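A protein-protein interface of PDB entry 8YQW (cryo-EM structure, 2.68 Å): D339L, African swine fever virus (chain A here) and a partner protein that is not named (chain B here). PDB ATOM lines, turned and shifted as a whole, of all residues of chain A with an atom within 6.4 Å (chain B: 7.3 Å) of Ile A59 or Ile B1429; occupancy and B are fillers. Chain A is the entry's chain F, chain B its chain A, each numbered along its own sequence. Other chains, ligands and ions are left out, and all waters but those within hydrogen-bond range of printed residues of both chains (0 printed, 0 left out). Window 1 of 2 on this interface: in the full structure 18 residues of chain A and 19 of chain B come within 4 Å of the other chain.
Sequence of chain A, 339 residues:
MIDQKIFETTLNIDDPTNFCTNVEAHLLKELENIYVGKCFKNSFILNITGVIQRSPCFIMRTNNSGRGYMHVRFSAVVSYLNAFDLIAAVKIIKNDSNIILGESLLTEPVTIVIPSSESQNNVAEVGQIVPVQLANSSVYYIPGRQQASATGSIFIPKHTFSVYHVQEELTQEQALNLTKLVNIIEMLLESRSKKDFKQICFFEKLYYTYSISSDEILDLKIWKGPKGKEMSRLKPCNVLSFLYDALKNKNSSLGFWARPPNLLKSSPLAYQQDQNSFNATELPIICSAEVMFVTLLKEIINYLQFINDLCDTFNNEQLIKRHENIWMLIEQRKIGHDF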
ATOM      1  N   PRO A  16      30.268  24.463 -11.484  1.00  0.00           N
ATOM      2  CA  PRO A  16      29.332  23.830 -10.544  1.00  0.00           C
ATOM      3  C   PRO A  16      29.905  22.624  -9.821  1.00  0.00           C
ATOM      4  O   PRO A  16      29.503  22.350  -8.685  1.00  0.00           O
ATOM      5  CB  PRO A  16      28.151  23.443 -11.445  1.00  0.00           C
ATOM      6  CG  PRO A  16      28.278  24.317 -12.640  1.00  0.00           C
ATOM      7  CD  PRO A  16      29.741  24.478 -12.855  1.00  0.00           C
ATOM      8  N   CYS A  57      21.611  23.854  -6.952  1.00  0.00           N
ATOM      9  CA  CYS A  57      22.393  24.442  -8.030  1.00  0.00           C
ATOM     10  C   CYS A  57      21.835  23.999  -9.374  1.00  0.00           C
ATOM     11  O   CYS A  57      22.197  22.933  -9.880  1.00  0.00           O
ATOM     12  CB  CYS A  57      23.867  24.061  -7.905  1.00  0.00           C
ATOM     13  SG  CYS A  57      24.941  24.826  -9.139  1.00  0.00           S
ATOM     14  N   PHE A  58      20.948  24.801  -9.954  1.00  0.00           N
ATOM     15  CA  PHE A  58      20.423  24.494 -11.271  1.00  0.00           C
ATOM     16  C   PHE A  58      21.495  24.723 -12.329  1.00  0.00           C
ATOM     17  O   PHE A  58      22.494  25.402 -12.097  1.00  0.00           O
ATOM     18  CB  PHE A  58      19.205  25.358 -11.591  1.00  0.00           C
ATOM     19  CG  PHE A  58      18.189  25.420 -10.494  1.00  0.00           C
ATOM     20  CD1 PHE A  58      17.268  24.406 -10.327  1.00  0.00           C
ATOM     21  CD2 PHE A  58      18.138  26.508  -9.645  1.00  0.00           C
ATOM     22  CE1 PHE A  58      16.328  24.470  -9.326  1.00  0.00           C
ATOM     23  CE2 PHE A  58      17.199  26.575  -8.645  1.00  0.00           C
ATOM     24  CZ  PHE A  58      16.294  25.554  -8.485  1.00  0.00           C
ATOM     25  N   ILE A  59      21.277  24.144 -13.503  1.00  0.00           N
ATOM     26  CA  ILE A  59      22.159  24.321 -14.650  1.00  0.00           C
ATOM     27  C   ILE A  59      21.464  25.247 -15.633  1.00  0.00           C
ATOM     28  O   ILE A  59      20.275  25.068 -15.924  1.00  0.00           O
ATOM     29  CB  ILE A  59      22.513  22.976 -15.307  1.00  0.00           C
ATOM     30  CG1 ILE A  59      23.161  22.045 -14.286  1.00  0.00           C
ATOM     31  CG2 ILE A  59      23.435  23.186 -16.487  1.00  0.00           C
ATOM     32  CD1 ILE A  59      24.410  22.603 -13.671  1.00  0.00           C
ATOM     33  N   MET A  60      22.193  26.246 -16.126  1.00  0.00           N
ATOM     34  CA  MET A  60      21.612  27.216 -17.043  1.00  0.00           C
ATOM     35  C   MET A  60      21.044  26.511 -18.263  1.00  0.00           C
ATOM     36  O   MET A  60      21.698  25.659 -18.868  1.00  0.00           O
ATOM     37  CB  MET A  60      22.658  28.244 -17.465  1.00  0.00           C
ATOM     38  CG  MET A  60      23.308  28.973 -16.313  1.00  0.00           C
ATOM     39  SD  MET A  60      24.440  30.247 -16.875  1.00  0.00           S
ATOM     40  CE  MET A  60      24.725  31.124 -15.348  1.00  0.00           C
ATOM     41  N   ARG A  61      19.820  26.877 -18.625  1.00  0.00           N
ATOM     42  CA  ARG A  61      19.046  26.149 -19.618  1.00  0.00           C
ATOM     43  C   ARG A  61      19.053  26.803 -20.989  1.00  0.00           C
ATOM     44  O   ARG A  61      18.874  26.108 -21.991  1.00  0.00           O
ATOM     45  CB  ARG A  61      17.600  26.007 -19.134  1.00  0.00           C
ATOM     46  CG  ARG A  61      16.770  24.996 -19.884  1.00  0.00           C
ATOM     47  CD  ARG A  61      15.297  25.151 -19.561  1.00  0.00           C
ATOM     48  NE  ARG A  61      14.784  26.458 -19.956  1.00  0.00           N
ATOM     49  CZ  ARG A  61      14.427  26.787 -21.190  1.00  0.00           C
ATOM     50  NH1 ARG A  61      14.527  25.928 -22.190  1.00  0.00           N
ATOM     51  NH2 ARG A  61      13.960  28.008 -21.427  1.00  0.00           N
ATOM     52  N   THR A  62      19.274  28.110 -21.065  1.00  0.00           N
ATOM     53  CA  THR A  62      19.131  28.847 -22.311  1.00  0.00           C
ATOM     54  C   THR A  62      20.453  29.073 -23.029  1.00  0.00           C
ATOM     55  O   THR A  62      20.495  29.848 -23.989  1.00  0.00           O
ATOM     56  CB  THR A  62      18.447  30.188 -22.049  1.00  0.00           C
ATOM     57  OG1 THR A  62      19.133  30.874 -20.997  1.00  0.00           O
ATOM     58  CG2 THR A  62      17.004  29.973 -21.642  1.00  0.00           C
ATOM     59  N   GLY A  66      26.991  25.218 -19.768  1.00  0.00           N
ATOM     60  CA  GLY A  66      27.105  24.244 -18.707  1.00  0.00           C
ATOM     61  C   GLY A  66      27.243  24.829 -17.322  1.00  0.00           C
ATOM     62  O   GLY A  66      27.439  24.070 -16.364  1.00  0.00           O
ATOM     63  N   ARG A  67      27.146  26.146 -17.183  1.00  0.00           N
ATOM     64  CA  ARG A  67      27.303  26.808 -15.903  1.00  0.00           C
ATOM     65  C   ARG A  67      26.021  26.693 -15.086  1.00  0.00           C
ATOM     66  O   ARG A  67      24.967  26.295 -15.585  1.00  0.00           O
ATOM     67  CB  ARG A  67      27.689  28.270 -16.112  1.00  0.00           C
ATOM     68  CG  ARG A  67      29.029  28.441 -16.799  1.00  0.00           C
ATOM     69  CD  ARG A  67      29.152  29.794 -17.462  1.00  0.00           C
ATOM     70  NE  ARG A  67      29.256  30.872 -16.489  1.00  0.00           N
ATOM     71  CZ  ARG A  67      28.643  32.041 -16.601  1.00  0.00           C
ATOM     72  NH1 ARG A  67      27.877  32.321 -17.642  1.00  0.00           N
ATOM     73  NH2 ARG A  67      28.803  32.952 -15.646  1.00  0.00           N
ATOM     74  N   GLY A  68      26.121  27.040 -13.802  1.00  0.00           N
ATOM     75  CA  GLY A  68      25.018  26.909 -12.883  1.00  0.00           C
ATOM     76  C   GLY A  68      24.562  28.251 -12.332  1.00  0.00           C
ATOM     77  O   GLY A  68      25.176  29.293 -12.566  1.00  0.00           O
ATOM     78  N   TYR A  69      23.466  28.206 -11.584  1.00  0.00           N
ATOM     79  CA  TYR A  69      22.978  29.379 -10.879  1.00  0.00           C
ATOM     80  C   TYR A  69      22.251  28.919  -9.627  1.00  0.00           C
ATOM     81  O   TYR A  69      21.813  27.772  -9.526  1.00  0.00           O
ATOM     82  CB  TYR A  69      22.069  30.240 -11.760  1.00  0.00           C
ATOM     83  CG  TYR A  69      20.797  29.556 -12.196  1.00  0.00           C
ATOM     84  CD1 TYR A  69      20.785  28.712 -13.292  1.00  0.00           C
ATOM     85  CD2 TYR A  69      19.608  29.768 -11.520  1.00  0.00           C
ATOM     86  CE1 TYR A  69      19.628  28.090 -13.696  1.00  0.00           C
ATOM     87  CE2 TYR A  69      18.448  29.150 -11.917  1.00  0.00           C
ATOM     88  CZ  TYR A  69      18.462  28.314 -13.006  1.00  0.00           C
ATOM     89  OH  TYR A  69      17.301  27.693 -13.403  1.00  0.00           O
ATOM     90  N   TYR B   5      21.487  34.950 -13.261  1.00  0.00           N
ATOM     91  CA  TYR B   5      20.801  34.296 -14.364  1.00  0.00           C
ATOM     92  C   TYR B   5      19.293  34.384 -14.178  1.00  0.00           C
ATOM     93  O   TYR B   5      18.777  34.220 -13.071  1.00  0.00           O
ATOM     94  CB  TYR B   5      21.238  32.834 -14.460  1.00  0.00           C
ATOM     95  CG  TYR B   5      20.507  32.021 -15.498  1.00  0.00           C
ATOM     96  CD1 TYR B   5      20.892  32.050 -16.829  1.00  0.00           C
ATOM     97  CD2 TYR B   5      19.438  31.215 -15.147  1.00  0.00           C
ATOM     98  CE1 TYR B   5      20.227  31.303 -17.776  1.00  0.00           C
ATOM     99  CE2 TYR B   5      18.772  30.468 -16.086  1.00  0.00           C
ATOM    100  CZ  TYR B   5      19.168  30.516 -17.396  1.00  0.00           C
ATOM    101  OH  TYR B   5      18.498  29.769 -18.331  1.00  0.00           O
ATOM    102  N   GLU B   7      15.205  34.149 -16.480  1.00  0.00           N
ATOM    103  CA  GLU B   7      14.414  33.794 -17.646  1.00  0.00           C
ATOM    104  C   GLU B   7      13.113  34.578 -17.606  1.00  0.00           C
ATOM    105  O   GLU B   7      12.680  35.037 -16.550  1.00  0.00           O
ATOM    106  CB  GLU B   7      14.117  32.291 -17.693  1.00  0.00           C
ATOM    107  CG  GLU B   7      15.332  31.426 -17.928  1.00  0.00           C
ATOM    108  CD  GLU B   7      15.007  29.951 -17.878  1.00  0.00           C
ATOM    109  OE1 GLU B   7      13.846  29.611 -17.572  1.00  0.00           O
ATOM    110  OE2 GLU B   7      15.910  29.129 -18.139  1.00  0.00           O
ATOM    111  N   MET B 472      27.847  20.413 -26.300  1.00  0.00           N
ATOM    112  CA  MET B 472      26.442  20.130 -26.015  1.00  0.00           C
ATOM    113  C   MET B 472      25.674  19.763 -27.279  1.00  0.00           C
ATOM    114  O   MET B 472      24.885  18.814 -27.278  1.00  0.00           O
ATOM    115  CB  MET B 472      25.796  21.332 -25.334  1.00  0.00           C
ATOM    116  CG  MET B 472      26.216  21.539 -23.899  1.00  0.00           C
ATOM    117  SD  MET B 472      24.900  22.278 -22.926  1.00  0.00           S
ATOM    118  CE  MET B 472      25.496  21.976 -21.274  1.00  0.00           C
ATOM    119  N   THR B1424      15.095  18.130 -24.813  1.00  0.00           N
ATOM    120  CA  THR B1424      16.204  18.102 -23.867  1.00  0.00           C
ATOM    121  C   THR B1424      16.100  19.196 -22.818  1.00  0.00           C
ATOM    122  O   THR B1424      16.703  19.070 -21.749  1.00  0.00           O
ATOM    123  CB  THR B1424      17.537  18.220 -24.604  1.00  0.00           C
ATOM    124  OG1 THR B1424      17.513  19.365 -25.461  1.00  0.00           O
ATOM    125  CG2 THR B1424      17.796  16.985 -25.429  1.00  0.00           C
ATOM    126  N   SER B1427      13.121  18.800 -18.830  1.00  0.00           N
ATOM    127  CA  SER B1427      13.503  18.557 -17.448  1.00  0.00           C
ATOM    128  C   SER B1427      14.804  19.288 -17.163  1.00  0.00           C
ATOM    129  O   SER B1427      15.738  19.239 -17.971  1.00  0.00           O
ATOM    130  CB  SER B1427      13.665  17.062 -17.173  1.00  0.00           C
ATOM    131  OG  SER B1427      12.466  16.360 -17.437  1.00  0.00           O
ATOM    132  N   ASP B1428      14.867  19.966 -16.024  1.00  0.00           N
ATOM    133  CA  ASP B1428      16.051  20.721 -15.659  1.00  0.00           C
ATOM    134  C   ASP B1428      16.980  19.880 -14.793  1.00  0.00           C
ATOM    135  O   ASP B1428      16.543  18.997 -14.052  1.00  0.00           O
ATOM    136  CB  ASP B1428      15.675  22.031 -14.955  1.00  0.00           C
ATOM    137  CG  ASP B1428      14.727  21.831 -13.795  1.00  0.00           C
ATOM    138  OD1 ASP B1428      14.886  20.856 -13.042  1.00  0.00           O
ATOM    139  OD2 ASP B1428      13.811  22.661 -13.633  1.00  0.00           O
ATOM    140  N   ILE B1429      18.273  20.144 -14.920  1.00  0.00           N
ATOM    141  CA  ILE B1429      19.310  19.385 -14.234  1.00  0.00           C
ATOM    142  C   ILE B1429      19.813  20.205 -13.060  1.00  0.00           C
ATOM    143  O   ILE B1429      19.979  21.426 -13.166  1.00  0.00           O
ATOM    144  CB  ILE B1429      20.462  19.024 -15.192  1.00  0.00           C
ATOM    145  CG1 ILE B1429      19.916  18.486 -16.514  1.00  0.00           C
ATOM    146  CG2 ILE B1429      21.379  18.004 -14.560  1.00  0.00           C
ATOM    147  CD1 ILE B1429      19.060  17.254 -16.370  1.00  0.00           C
ATOM    148  N   ILE B1430      20.036  19.543 -11.931  1.00  0.00           N
ATOM    149  CA  ILE B1430      20.624  20.178 -10.760  1.00  0.00           C
ATOM    150  C   ILE B1430      21.829  19.360 -10.328  1.00  0.00           C
ATOM    151  O   ILE B1430      21.862  18.136 -10.479  1.00  0.00           O
ATOM    152  CB  ILE B1430      19.616  20.332  -9.599  1.00  0.00           C
ATOM    153  CG1 ILE B1430      19.181  18.970  -9.067  1.00  0.00           C
ATOM    154  CG2 ILE B1430      18.411  21.124 -10.044  1.00  0.00           C
ATOM    155  CD1 ILE B1430      18.372  19.046  -7.808  1.00  0.00           C
ATOM    156  N   MET B1431      22.835  20.052  -9.803  1.00  0.00           N
ATOM    157  CA  MET B1431      24.052  19.395  -9.357  1.00  0.00           C
ATOM    158  C   MET B1431      23.768  18.551  -8.123  1.00  0.00           C
ATOM    159  O   MET B1431      23.051  18.976  -7.215  1.00  0.00           O
ATOM    160  CB  MET B1431      25.130  20.431  -9.047  1.00  0.00           C
ATOM    161  CG  MET B1431      25.558  21.266 -10.238  1.00  0.00           C
ATOM    162  SD  MET B1431      26.283  20.320 -11.582  1.00  0.00           S
ATOM    163  CE  MET B1431      27.564  19.426 -10.720  1.00  0.00           C
ATOM    164  N   ASP B1432      24.334  17.347  -8.094  1.00  0.00           N
ATOM    165  CA  ASP B1432      24.156  16.441  -6.962  1.00  0.00           C
ATOM    166  C   ASP B1432      25.076  16.897  -5.838  1.00  0.00           C
ATOM    167  O   ASP B1432      26.255  16.541  -5.799  1.00  0.00           O
ATOM    168  CB  ASP B1432      24.443  15.003  -7.371  1.00  0.00           C
ATOM    169  CG  ASP B1432      23.769  13.999  -6.467  1.00  0.00           C
ATOM    170  OD1 ASP B1432      23.390  14.375  -5.339  1.00  0.00           O
ATOM    171  OD2 ASP B1432      23.614  12.834  -6.880  1.00  0.00           O
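The side-chain hydroxyl of Tyr B5 lies within hydrogen-bond range of the backbone NH of Arg A61 (3.2 Å). The side-chain hydroxyl of Tyr B5 is in hydrogen-bond range of the side-chain hydroxyl of Thr A62, 3.0 Å away. NE of Arg A61 is in salt-bridge range of OE2 of Glu B7 (3.4 Å). O of Ile B1429 is in hydrogen-bond range of N of Ile A59 (3.0 Å). O of Cys A57 lies within hydrogen-bond range of N of Met B1431, 3.0 Å away.
OH of Tyr B5 sits at hydrogen-bond distance from OE2 of Glu B7, 2.7 Å away. The backbone NH of Tyr A69 is in hydrogen-bond range of the backbone carbonyl oxygen of Phe A58 (3.0 Å). O of Arg A67 sits at hydrogen-bond distance from N of Met A60 (2.8 Å).
Among the printed residues, pairs that only touch across the chains: Cys A57 with Ile B1430 (3.3 Å), Tyr A69 with Tyr B5 (3.4 Å), Phe A58 with Ile B1430 (3.5 Å), Pro A16 with Met B1431 (3.6 Å), Ile A59 with Met B1431 (3.6 Å), Phe A58 with Ile B1429 (3.6 Å), Thr A62 with Glu B7 (3.8 Å), Gly A66 with Met B472 (3.8 Å) and Met A60 with Tyr B5 (3.9 Å).
Ile A59 touches two residues of chain B. Of chain A, only Phe A58 and Ile A59 come within 4 Å of Ile B1429. Printed residues of chain B within 4 Å of Cys A57: Ile B1430 and Met B1431. Printed residues of chain A within 4 Å of Met B1431: Pro A16 (3.6 Å), Cys A57 (3.0 Å) and Ile A59 (3.6 Å). Of the printed residues of chain A, Glu B7 touches Arg A61 and Thr A62. Printed residues of chain A within 4 Å of Met B472: Gly A66 (3.8 Å). Of the printed residues of chain A, Tyr B5 touches Met A60 (3.9 Å), Arg A61 (3.2 Å), Thr A62 (3.0 Å) and Tyr A69 (3.4 Å). Ser B1427 touches none of the printed residues of chain A. The nearest residue of chain B that does not touch Ile A59 is Ile B1430 (4.6 Å). The nearest residue of chain A that does not touch Ile B1429 is Cys A57 (4.2 Å). The nearest printed residue of chain B that does not touch Thr A62 is Met B472 (8.1 Å).
Of the 10 printed residues of chain B, 6 touch a printed residue of chain A. Printed residues of chain B that touch a printed residue of chain A: Tyr B5, Glu B7, Met B472, Ile B1429, Ile B1430 and Met B1431. Of the 11 printed residues of chain A, 9 touch a printed residue of chain B. Printed residues of chain A that touch a printed residue of chain B: Pro A16, Cys A57, Phe A58, Ile A59, Met A60, Arg A61, Thr A62, Gly A66 and Tyr A69. Among the printed residues, 14 pairs touch across the chains.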
